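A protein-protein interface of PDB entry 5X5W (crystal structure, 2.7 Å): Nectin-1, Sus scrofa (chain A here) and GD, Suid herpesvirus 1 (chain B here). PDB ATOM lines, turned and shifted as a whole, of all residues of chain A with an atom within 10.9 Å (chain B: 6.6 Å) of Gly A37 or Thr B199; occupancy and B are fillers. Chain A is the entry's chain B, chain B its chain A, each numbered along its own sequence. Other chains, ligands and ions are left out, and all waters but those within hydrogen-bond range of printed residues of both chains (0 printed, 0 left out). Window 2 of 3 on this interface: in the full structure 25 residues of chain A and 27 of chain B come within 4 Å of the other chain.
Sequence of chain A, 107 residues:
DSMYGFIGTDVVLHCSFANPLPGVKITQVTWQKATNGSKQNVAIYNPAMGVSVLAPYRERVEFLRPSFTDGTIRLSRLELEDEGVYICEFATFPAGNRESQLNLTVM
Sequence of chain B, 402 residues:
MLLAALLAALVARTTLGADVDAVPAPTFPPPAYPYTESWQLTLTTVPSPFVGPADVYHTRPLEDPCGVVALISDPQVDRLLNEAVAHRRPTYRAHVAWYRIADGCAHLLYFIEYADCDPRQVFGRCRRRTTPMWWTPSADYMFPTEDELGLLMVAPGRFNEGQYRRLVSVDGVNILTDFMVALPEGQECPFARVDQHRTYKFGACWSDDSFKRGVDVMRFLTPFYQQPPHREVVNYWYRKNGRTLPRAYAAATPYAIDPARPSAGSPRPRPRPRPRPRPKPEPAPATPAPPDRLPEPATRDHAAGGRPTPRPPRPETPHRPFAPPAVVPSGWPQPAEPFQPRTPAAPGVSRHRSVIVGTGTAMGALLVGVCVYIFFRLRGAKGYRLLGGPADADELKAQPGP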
ATOM      1  N   GLN A  32       3.094  14.817   3.426  1.00  0.00           N
ATOM      2  CA  GLN A  32       2.662  14.816   4.799  1.00  0.00           C
ATOM      3  C   GLN A  32       1.299  15.409   4.932  1.00  0.00           C
ATOM      4  O   GLN A  32       1.006  16.355   4.293  1.00  0.00           O
ATOM      5  CB  GLN A  32       3.613  15.644   5.638  1.00  0.00           C
ATOM      6  CG  GLN A  32       5.011  15.113   5.641  1.00  0.00           C
ATOM      7  CD  GLN A  32       5.951  15.985   6.382  1.00  0.00           C
ATOM      8  OE1 GLN A  32       5.754  17.165   6.466  1.00  0.00           O
ATOM      9  NE2 GLN A  32       6.976  15.397   6.937  1.00  0.00           N
ATOM     10  N   LYS A  33       0.470  14.854   5.787  1.00  0.00           N
ATOM     11  CA  LYS A  33      -0.821  15.455   6.108  1.00  0.00           C
ATOM     12  C   LYS A  33      -0.838  16.023   7.519  1.00  0.00           C
ATOM     13  O   LYS A  33      -0.388  15.379   8.466  1.00  0.00           O
ATOM     14  CB  LYS A  33      -1.968  14.457   5.953  1.00  0.00           C
ATOM     15  CG  LYS A  33      -3.307  15.094   6.295  1.00  0.00           C
ATOM     16  CD  LYS A  33      -4.490  14.246   5.904  1.00  0.00           C
ATOM     17  CE  LYS A  33      -5.783  14.991   6.172  1.00  0.00           C
ATOM     18  NZ  LYS A  33      -6.957  14.106   5.963  1.00  0.00           N
ATOM     19  N   ALA A  34      -1.358  17.239   7.645  1.00  0.00           N
ATOM     20  CA  ALA A  34      -1.540  17.870   8.941  1.00  0.00           C
ATOM     21  C   ALA A  34      -2.888  17.469   9.528  1.00  0.00           C
ATOM     22  O   ALA A  34      -3.939  17.792   8.964  1.00  0.00           O
ATOM     23  CB  ALA A  34      -1.440  19.375   8.816  1.00  0.00           C
ATOM     24  N   THR A  35      -2.860  16.735  10.614  1.00  0.00           N
ATOM     25  CA  THR A  35      -4.060  16.175  11.150  1.00  0.00           C
ATOM     26  C   THR A  35      -3.894  16.063  12.602  1.00  0.00           C
ATOM     27  O   THR A  35      -2.897  15.593  13.065  1.00  0.00           O
ATOM     28  CB  THR A  35      -4.272  14.719  10.718  1.00  0.00           C
ATOM     29  OG1 THR A  35      -3.147  13.948  11.095  1.00  0.00           O
ATOM     30  CG2 THR A  35      -4.420  14.602   9.246  1.00  0.00           C
ATOM     31  N   ASN A  36      -4.918  16.408  13.342  1.00  0.00           N
ATOM     32  CA  ASN A  36      -4.958  16.072  14.748  1.00  0.00           C
ATOM     33  C   ASN A  36      -4.035  16.918  15.538  1.00  0.00           C
ATOM     34  O   ASN A  36      -4.073  16.915  16.747  1.00  0.00           O
ATOM     35  CB  ASN A  36      -4.582  14.621  14.955  1.00  0.00           C
ATOM     36  CG  ASN A  36      -5.720  13.795  15.406  1.00  0.00           C
ATOM     37  OD1 ASN A  36      -5.511  12.765  15.992  1.00  0.00           O
ATOM     38  ND2 ASN A  36      -6.927  14.237  15.158  1.00  0.00           N
ATOM     39  N   GLY A  37      -3.118  17.588  14.877  1.00  0.00           N
ATOM     40  CA  GLY A  37      -2.208  18.396  15.637  1.00  0.00           C
ATOM     41  C   GLY A  37      -0.829  18.424  15.096  1.00  0.00           C
ATOM     42  O   GLY A  37      -0.105  19.324  15.384  1.00  0.00           O
ATOM     43  N   SER A  38      -0.465  17.435  14.324  1.00  0.00           N
ATOM     44  CA  SER A  38       0.839  17.430  13.705  1.00  0.00           C
ATOM     45  C   SER A  38       0.813  16.780  12.344  1.00  0.00           C
ATOM     46  O   SER A  38      -0.190  16.791  11.678  1.00  0.00           O
ATOM     47  CB  SER A  38       1.897  16.790  14.613  1.00  0.00           C
ATOM     48  OG  SER A  38       1.370  15.800  15.433  1.00  0.00           O
ATOM     49  N   LYS A  39       1.937  16.237  11.941  1.00  0.00           N
ATOM     50  CA  LYS A  39       2.004  15.578  10.690  1.00  0.00           C
ATOM     51  C   LYS A  39       2.174  14.146  10.928  1.00  0.00           C
ATOM     52  O   LYS A  39       2.499  13.739  11.987  1.00  0.00           O
ATOM     53  CB  LYS A  39       3.130  16.102   9.824  1.00  0.00           C
ATOM     54  CG  LYS A  39       3.641  17.465  10.165  1.00  0.00           C
ATOM     55  CD  LYS A  39       5.140  17.391  10.305  1.00  0.00           C
ATOM     56  CE  LYS A  39       5.809  18.638   9.807  1.00  0.00           C
ATOM     57  NZ  LYS A  39       6.387  18.494   8.450  1.00  0.00           N
ATOM     58  N   GLN A  40       1.884  13.398   9.894  1.00  0.00           N
ATOM     59  CA  GLN A  40       2.289  12.052   9.739  1.00  0.00           C
ATOM     60  C   GLN A  40       2.625  12.019   8.286  1.00  0.00           C
ATOM     61  O   GLN A  40       2.091  12.756   7.541  1.00  0.00           O
ATOM     62  CB  GLN A  40       1.177  11.068  10.095  1.00  0.00           C
ATOM     63  CG  GLN A  40      -0.173  11.672  10.375  1.00  0.00           C
ATOM     64  CD  GLN A  40      -0.821  11.138  11.617  1.00  0.00           C
ATOM     65  OE1 GLN A  40      -1.361  10.060  11.620  1.00  0.00           O
ATOM     66  NE2 GLN A  40      -0.792  11.913  12.668  1.00  0.00           N
ATOM     67  N   GLY A  84      -8.093  18.685   4.043  1.00  0.00           N
ATOM     68  CA  GLY A  84      -7.088  19.254   4.920  1.00  0.00           C
ATOM     69  C   GLY A  84      -5.807  19.692   4.238  1.00  0.00           C
ATOM     70  O   GLY A  84      -5.702  19.681   3.006  1.00  0.00           O
ATOM     71  N   VAL A  85      -4.826  20.076   5.052  1.00  0.00           N
ATOM     72  CA  VAL A  85      -3.548  20.564   4.549  1.00  0.00           C
ATOM     73  C   VAL A  85      -2.592  19.420   4.239  1.00  0.00           C
ATOM     74  O   VAL A  85      -2.418  18.502   5.046  1.00  0.00           O
ATOM     75  CB  VAL A  85      -2.877  21.511   5.556  1.00  0.00           C
ATOM     76  CG1 VAL A  85      -1.554  22.017   5.008  1.00  0.00           C
ATOM     77  CG2 VAL A  85      -3.809  22.665   5.892  1.00  0.00           C
ATOM     78  N   TYR A  86      -1.976  19.471   3.063  1.00  0.00           N
ATOM     79  CA  TYR A  86      -0.967  18.491   2.689  1.00  0.00           C
ATOM     80  C   TYR A  86       0.359  19.204   2.519  1.00  0.00           C
ATOM     81  O   TYR A  86       0.443  20.167   1.766  1.00  0.00           O
ATOM     82  CB  TYR A  86      -1.373  17.758   1.408  1.00  0.00           C
ATOM     83  CG  TYR A  86      -2.510  16.779   1.625  1.00  0.00           C
ATOM     84  CD1 TYR A  86      -2.278  15.410   1.641  1.00  0.00           C
ATOM     85  CD2 TYR A  86      -3.806  17.223   1.844  1.00  0.00           C
ATOM     86  CE1 TYR A  86      -3.303  14.516   1.848  1.00  0.00           C
ATOM     87  CE2 TYR A  86      -4.838  16.335   2.057  1.00  0.00           C
ATOM     88  CZ  TYR A  86      -4.580  14.980   2.056  1.00  0.00           C
ATOM     89  OH  TYR A  86      -5.602  14.080   2.263  1.00  0.00           O
ATOM     90  N   ILE A  87       1.387  18.763   3.237  1.00  0.00           N
ATOM     91  CA  ILE A  87       2.692  19.414   3.160  1.00  0.00           C
ATOM     92  C   ILE A  87       3.617  18.630   2.240  1.00  0.00           C
ATOM     93  O   ILE A  87       3.644  17.404   2.266  1.00  0.00           O
ATOM     94  CB  ILE A  87       3.365  19.563   4.553  1.00  0.00           C
ATOM     95  CG1 ILE A  87       2.505  20.417   5.490  1.00  0.00           C
ATOM     96  CG2 ILE A  87       4.750  20.175   4.418  1.00  0.00           C
ATOM     97  CD1 ILE A  87       1.645  19.604   6.450  1.00  0.00           C
ATOM     98  N   GLU A  99       9.654  23.246   2.555  1.00  0.00           N
ATOM     99  CA  GLU A  99       8.336  22.668   2.327  1.00  0.00           C
ATOM    100  C   GLU A  99       7.349  23.517   1.559  1.00  0.00           C
ATOM    101  O   GLU A  99       7.508  24.684   1.450  1.00  0.00           O
ATOM    102  CB  GLU A  99       7.726  22.311   3.656  1.00  0.00           C
ATOM    103  CG  GLU A  99       7.362  23.497   4.501  1.00  0.00           C
ATOM    104  CD  GLU A  99       6.916  23.088   5.859  1.00  0.00           C
ATOM    105  OE1 GLU A  99       5.790  23.409   6.224  1.00  0.00           O
ATOM    106  OE2 GLU A  99       7.678  22.417   6.559  1.00  0.00           O
ATOM    107  N   GLN A 101       2.794  23.723   0.714  1.00  0.00           N
ATOM    108  CA  GLN A 101       1.540  23.295   1.259  1.00  0.00           C
ATOM    109  C   GLN A 101       0.367  23.471   0.358  1.00  0.00           C
ATOM    110  O   GLN A 101       0.325  24.377  -0.409  1.00  0.00           O
ATOM    111  CB  GLN A 101       1.270  24.120   2.476  1.00  0.00           C
ATOM    112  CG  GLN A 101       2.199  23.831   3.605  1.00  0.00           C
ATOM    113  CD  GLN A 101       1.900  24.674   4.782  1.00  0.00           C
ATOM    114  OE1 GLN A 101       0.815  25.187   4.915  1.00  0.00           O
ATOM    115  NE2 GLN A 101       2.860  24.827   5.643  1.00  0.00           N
ATOM    116  N   VAL B 194      11.593  28.858  15.883  1.00  0.00           N
ATOM    117  CA  VAL B 194      10.371  28.739  16.671  1.00  0.00           C
ATOM    118  C   VAL B 194       9.100  28.626  15.822  1.00  0.00           C
ATOM    119  O   VAL B 194       7.998  28.558  16.364  1.00  0.00           O
ATOM    120  CB  VAL B 194      10.201  29.940  17.621  1.00  0.00           C
ATOM    121  CG1 VAL B 194      11.327  29.978  18.647  1.00  0.00           C
ATOM    122  CG2 VAL B 194      10.135  31.239  16.829  1.00  0.00           C
ATOM    123  N   ASP B 195       9.247  28.597  14.500  1.00  0.00           N
ATOM    124  CA  ASP B 195       8.093  28.674  13.607  1.00  0.00           C
ATOM    125  C   ASP B 195       7.324  27.357  13.524  1.00  0.00           C
ATOM    126  O   ASP B 195       6.118  27.332  13.763  1.00  0.00           O
ATOM    127  CB  ASP B 195       8.530  29.128  12.207  1.00  0.00           C
ATOM    128  CG  ASP B 195       9.843  28.499  11.768  1.00  0.00           C
ATOM    129  OD1 ASP B 195      10.657  28.141  12.649  1.00  0.00           O
ATOM    130  OD2 ASP B 195      10.063  28.369  10.544  1.00  0.00           O
ATOM    131  N   GLN B 196       8.020  26.272  13.192  1.00  0.00           N
ATOM    132  CA  GLN B 196       7.398  24.956  13.069  1.00  0.00           C
ATOM    133  C   GLN B 196       6.703  24.533  14.360  1.00  0.00           C
ATOM    134  O   GLN B 196       5.650  23.888  14.327  1.00  0.00           O
ATOM    135  CB  GLN B 196       8.434  23.892  12.688  1.00  0.00           C
ATOM    136  CG  GLN B 196       9.178  24.133  11.382  1.00  0.00           C
ATOM    137  CD  GLN B 196       8.276  24.102  10.163  1.00  0.00           C
ATOM    138  OE1 GLN B 196       7.455  23.192   9.994  1.00  0.00           O
ATOM    139  NE2 GLN B 196       8.426  25.101   9.300  1.00  0.00           N
ATOM    140  N   HIS B 197       7.301  24.899  15.491  1.00  0.00           N
ATOM    141  CA  HIS B 197       6.788  24.525  16.802  1.00  0.00           C
ATOM    142  C   HIS B 197       5.396  25.083  17.045  1.00  0.00           C
ATOM    143  O   HIS B 197       4.526  24.387  17.569  1.00  0.00           O
ATOM    144  CB  HIS B 197       7.729  25.007  17.903  1.00  0.00           C
ATOM    145  CG  HIS B 197       7.380  24.479  19.258  1.00  0.00           C
ATOM    146  ND1 HIS B 197       7.707  23.204  19.663  1.00  0.00           N
ATOM    147  CD2 HIS B 197       6.711  25.043  20.292  1.00  0.00           C
ATOM    148  CE1 HIS B 197       7.264  23.008  20.892  1.00  0.00           C
ATOM    149  NE2 HIS B 197       6.657  24.109  21.296  1.00  0.00           N
ATOM    150  N   ARG B 198       5.192  26.339  16.663  1.00  0.00           N
ATOM    151  CA  ARG B 198       3.871  26.960  16.713  1.00  0.00           C
ATOM    152  C   ARG B 198       2.804  26.079  16.075  1.00  0.00           C
ATOM    153  O   ARG B 198       1.686  25.973  16.583  1.00  0.00           O
ATOM    154  CB  ARG B 198       3.880  28.317  16.008  1.00  0.00           C
ATOM    155  CG  ARG B 198       4.670  29.384  16.720  1.00  0.00           C
ATOM    156  CD  ARG B 198       4.411  30.749  16.102  1.00  0.00           C
ATOM    157  NE  ARG B 198       4.890  31.821  16.969  1.00  0.00           N
ATOM    158  CZ  ARG B 198       4.208  32.303  18.003  1.00  0.00           C
ATOM    159  NH1 ARG B 198       3.010  31.811  18.303  1.00  0.00           N
ATOM    160  NH2 ARG B 198       4.723  33.278  18.741  1.00  0.00           N
ATOM    161  N   THR B 199       3.162  25.440  14.966  1.00  0.00           N
ATOM    162  CA  THR B 199       2.188  24.708  14.169  1.00  0.00           C
ATOM    163  C   THR B 199       2.062  23.229  14.549  1.00  0.00           C
ATOM    164  O   THR B 199       0.953  22.708  14.637  1.00  0.00           O
ATOM    165  CB  THR B 199       2.527  24.803  12.669  1.00  0.00           C
ATOM    166  OG1 THR B 199       3.011  26.118  12.370  1.00  0.00           O
ATOM    167  CG2 THR B 199       1.291  24.522  11.833  1.00  0.00           C
ATOM    168  N   TYR B 200       3.191  22.560  14.777  1.00  0.00           N
ATOM    169  CA  TYR B 200       3.187  21.114  14.995  1.00  0.00           C
ATOM    170  C   TYR B 200       3.624  20.702  16.396  1.00  0.00           C
ATOM    171  O   TYR B 200       3.288  19.606  16.857  1.00  0.00           O
ATOM    172  CB  TYR B 200       4.093  20.424  13.978  1.00  0.00           C
ATOM    173  CG  TYR B 200       3.787  20.790  12.551  1.00  0.00           C
ATOM    174  CD1 TYR B 200       2.558  20.483  11.986  1.00  0.00           C
ATOM    175  CD2 TYR B 200       4.727  21.440  11.766  1.00  0.00           C
ATOM    176  CE1 TYR B 200       2.272  20.812  10.681  1.00  0.00           C
ATOM    177  CE2 TYR B 200       4.449  21.778  10.457  1.00  0.00           C
ATOM    178  CZ  TYR B 200       3.221  21.459   9.920  1.00  0.00           C
ATOM    179  OH  TYR B 200       2.949  21.799   8.614  1.00  0.00           O
ATOM    180  N   LYS B 201       4.383  21.577  17.052  1.00  0.00           N
ATOM    181  CA  LYS B 201       4.959  21.301  18.373  1.00  0.00           C
ATOM    182  C   LYS B 201       5.853  20.068  18.374  1.00  0.00           C
ATOM    183  O   LYS B 201       6.724  19.924  17.516  1.00  0.00           O
ATOM    184  CB  LYS B 201       3.858  21.156  19.424  1.00  0.00           C
ATOM    185  CG  LYS B 201       3.128  22.455  19.675  1.00  0.00           C
ATOM    186  CD  LYS B 201       2.043  22.326  20.716  1.00  0.00           C
ATOM    187  CE  LYS B 201       1.324  23.655  20.874  1.00  0.00           C
ATOM    188  NZ  LYS B 201       0.290  23.611  21.941  1.00  0.00           N
ATOM    189  N   GLY B 203       4.857  16.854  18.289  1.00  0.00           N
ATOM    190  CA  GLY B 203       4.259  15.705  17.641  1.00  0.00           C
ATOM    191  C   GLY B 203       3.507  14.858  18.642  1.00  0.00           C
ATOM    192  O   GLY B 203       3.490  15.163  19.840  1.00  0.00           O
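The side-chain amide oxygen (OE1) of Gln A32 is in hydrogen-bond range of the side-chain amino group (NZ) of Lys A39 (2.5 Å). The backbone NH (N) of Ile A87 sits at hydrogen-bond distance from the backbone carbonyl oxygen (O) of Gln A32, at 2.7 Å. The side-chain carboxylate (OE1) of Glu A99 is in hydrogen-bond range of the side-chain amide nitrogen (NE2) of Gln A101 (3.3 Å).
Gly A37 touches Thr B199. Gly A37 touches Tyr B200 (O to O, 3.7 Å). Tyr B200 touches Ser A38. OG of Ser A38 touches CA of Gly B203 (3.6 Å). CE2 of Tyr B200 touches CE of Lys A39 (3.5 Å). OH of Tyr B200 touches CD1 of Ile A87 (3.3 Å). Gln B196 touches Glu A99 (OE1 to OE2, 3.5 Å).
Ala A34 touches none of the printed residues of chain B. Gly A37 touches two residues of chain B. Of the printed residues of chain B, Ser A38 touches Tyr B200 (3.9 Å) and Gly B203 (3.6 Å). Of the printed residues of chain B, Lys A39 touches Tyr B200. Of the printed residues of chain B, Ile A87 touches Tyr B200 (3.3 Å). Of the printed residues of chain B, Glu A99 touches Gln B196. Gln B196 touches just one residue of chain A: Glu A99 (3.5 Å). Thr B199 touches one residue of chain A. Printed residues of chain A within 4 Å of Gly B203: Ser A38. The nearest printed residue of chain B that does not touch Ile A87 is Gln B196 (6.9 Å).
Printed residues of chain A that touch a printed residue of chain B: Gly A37, Ser A38, Lys A39, Ile A87 and Glu A99. Hydrophobic or aromatic side chains of chain A within 4 Å of the printed part of chain B: Ile A87. Of the 9 printed residues of chain B, 4 touch a printed residue of chain A. Hydrophobic or aromatic side chains of chain B within 4 Å of the printed part of chain A: Tyr B200. Among the printed residues, no Asp or Glu carboxylate lies within 4 Å of a Lys or Arg side-chain nitrogen of the other chain.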
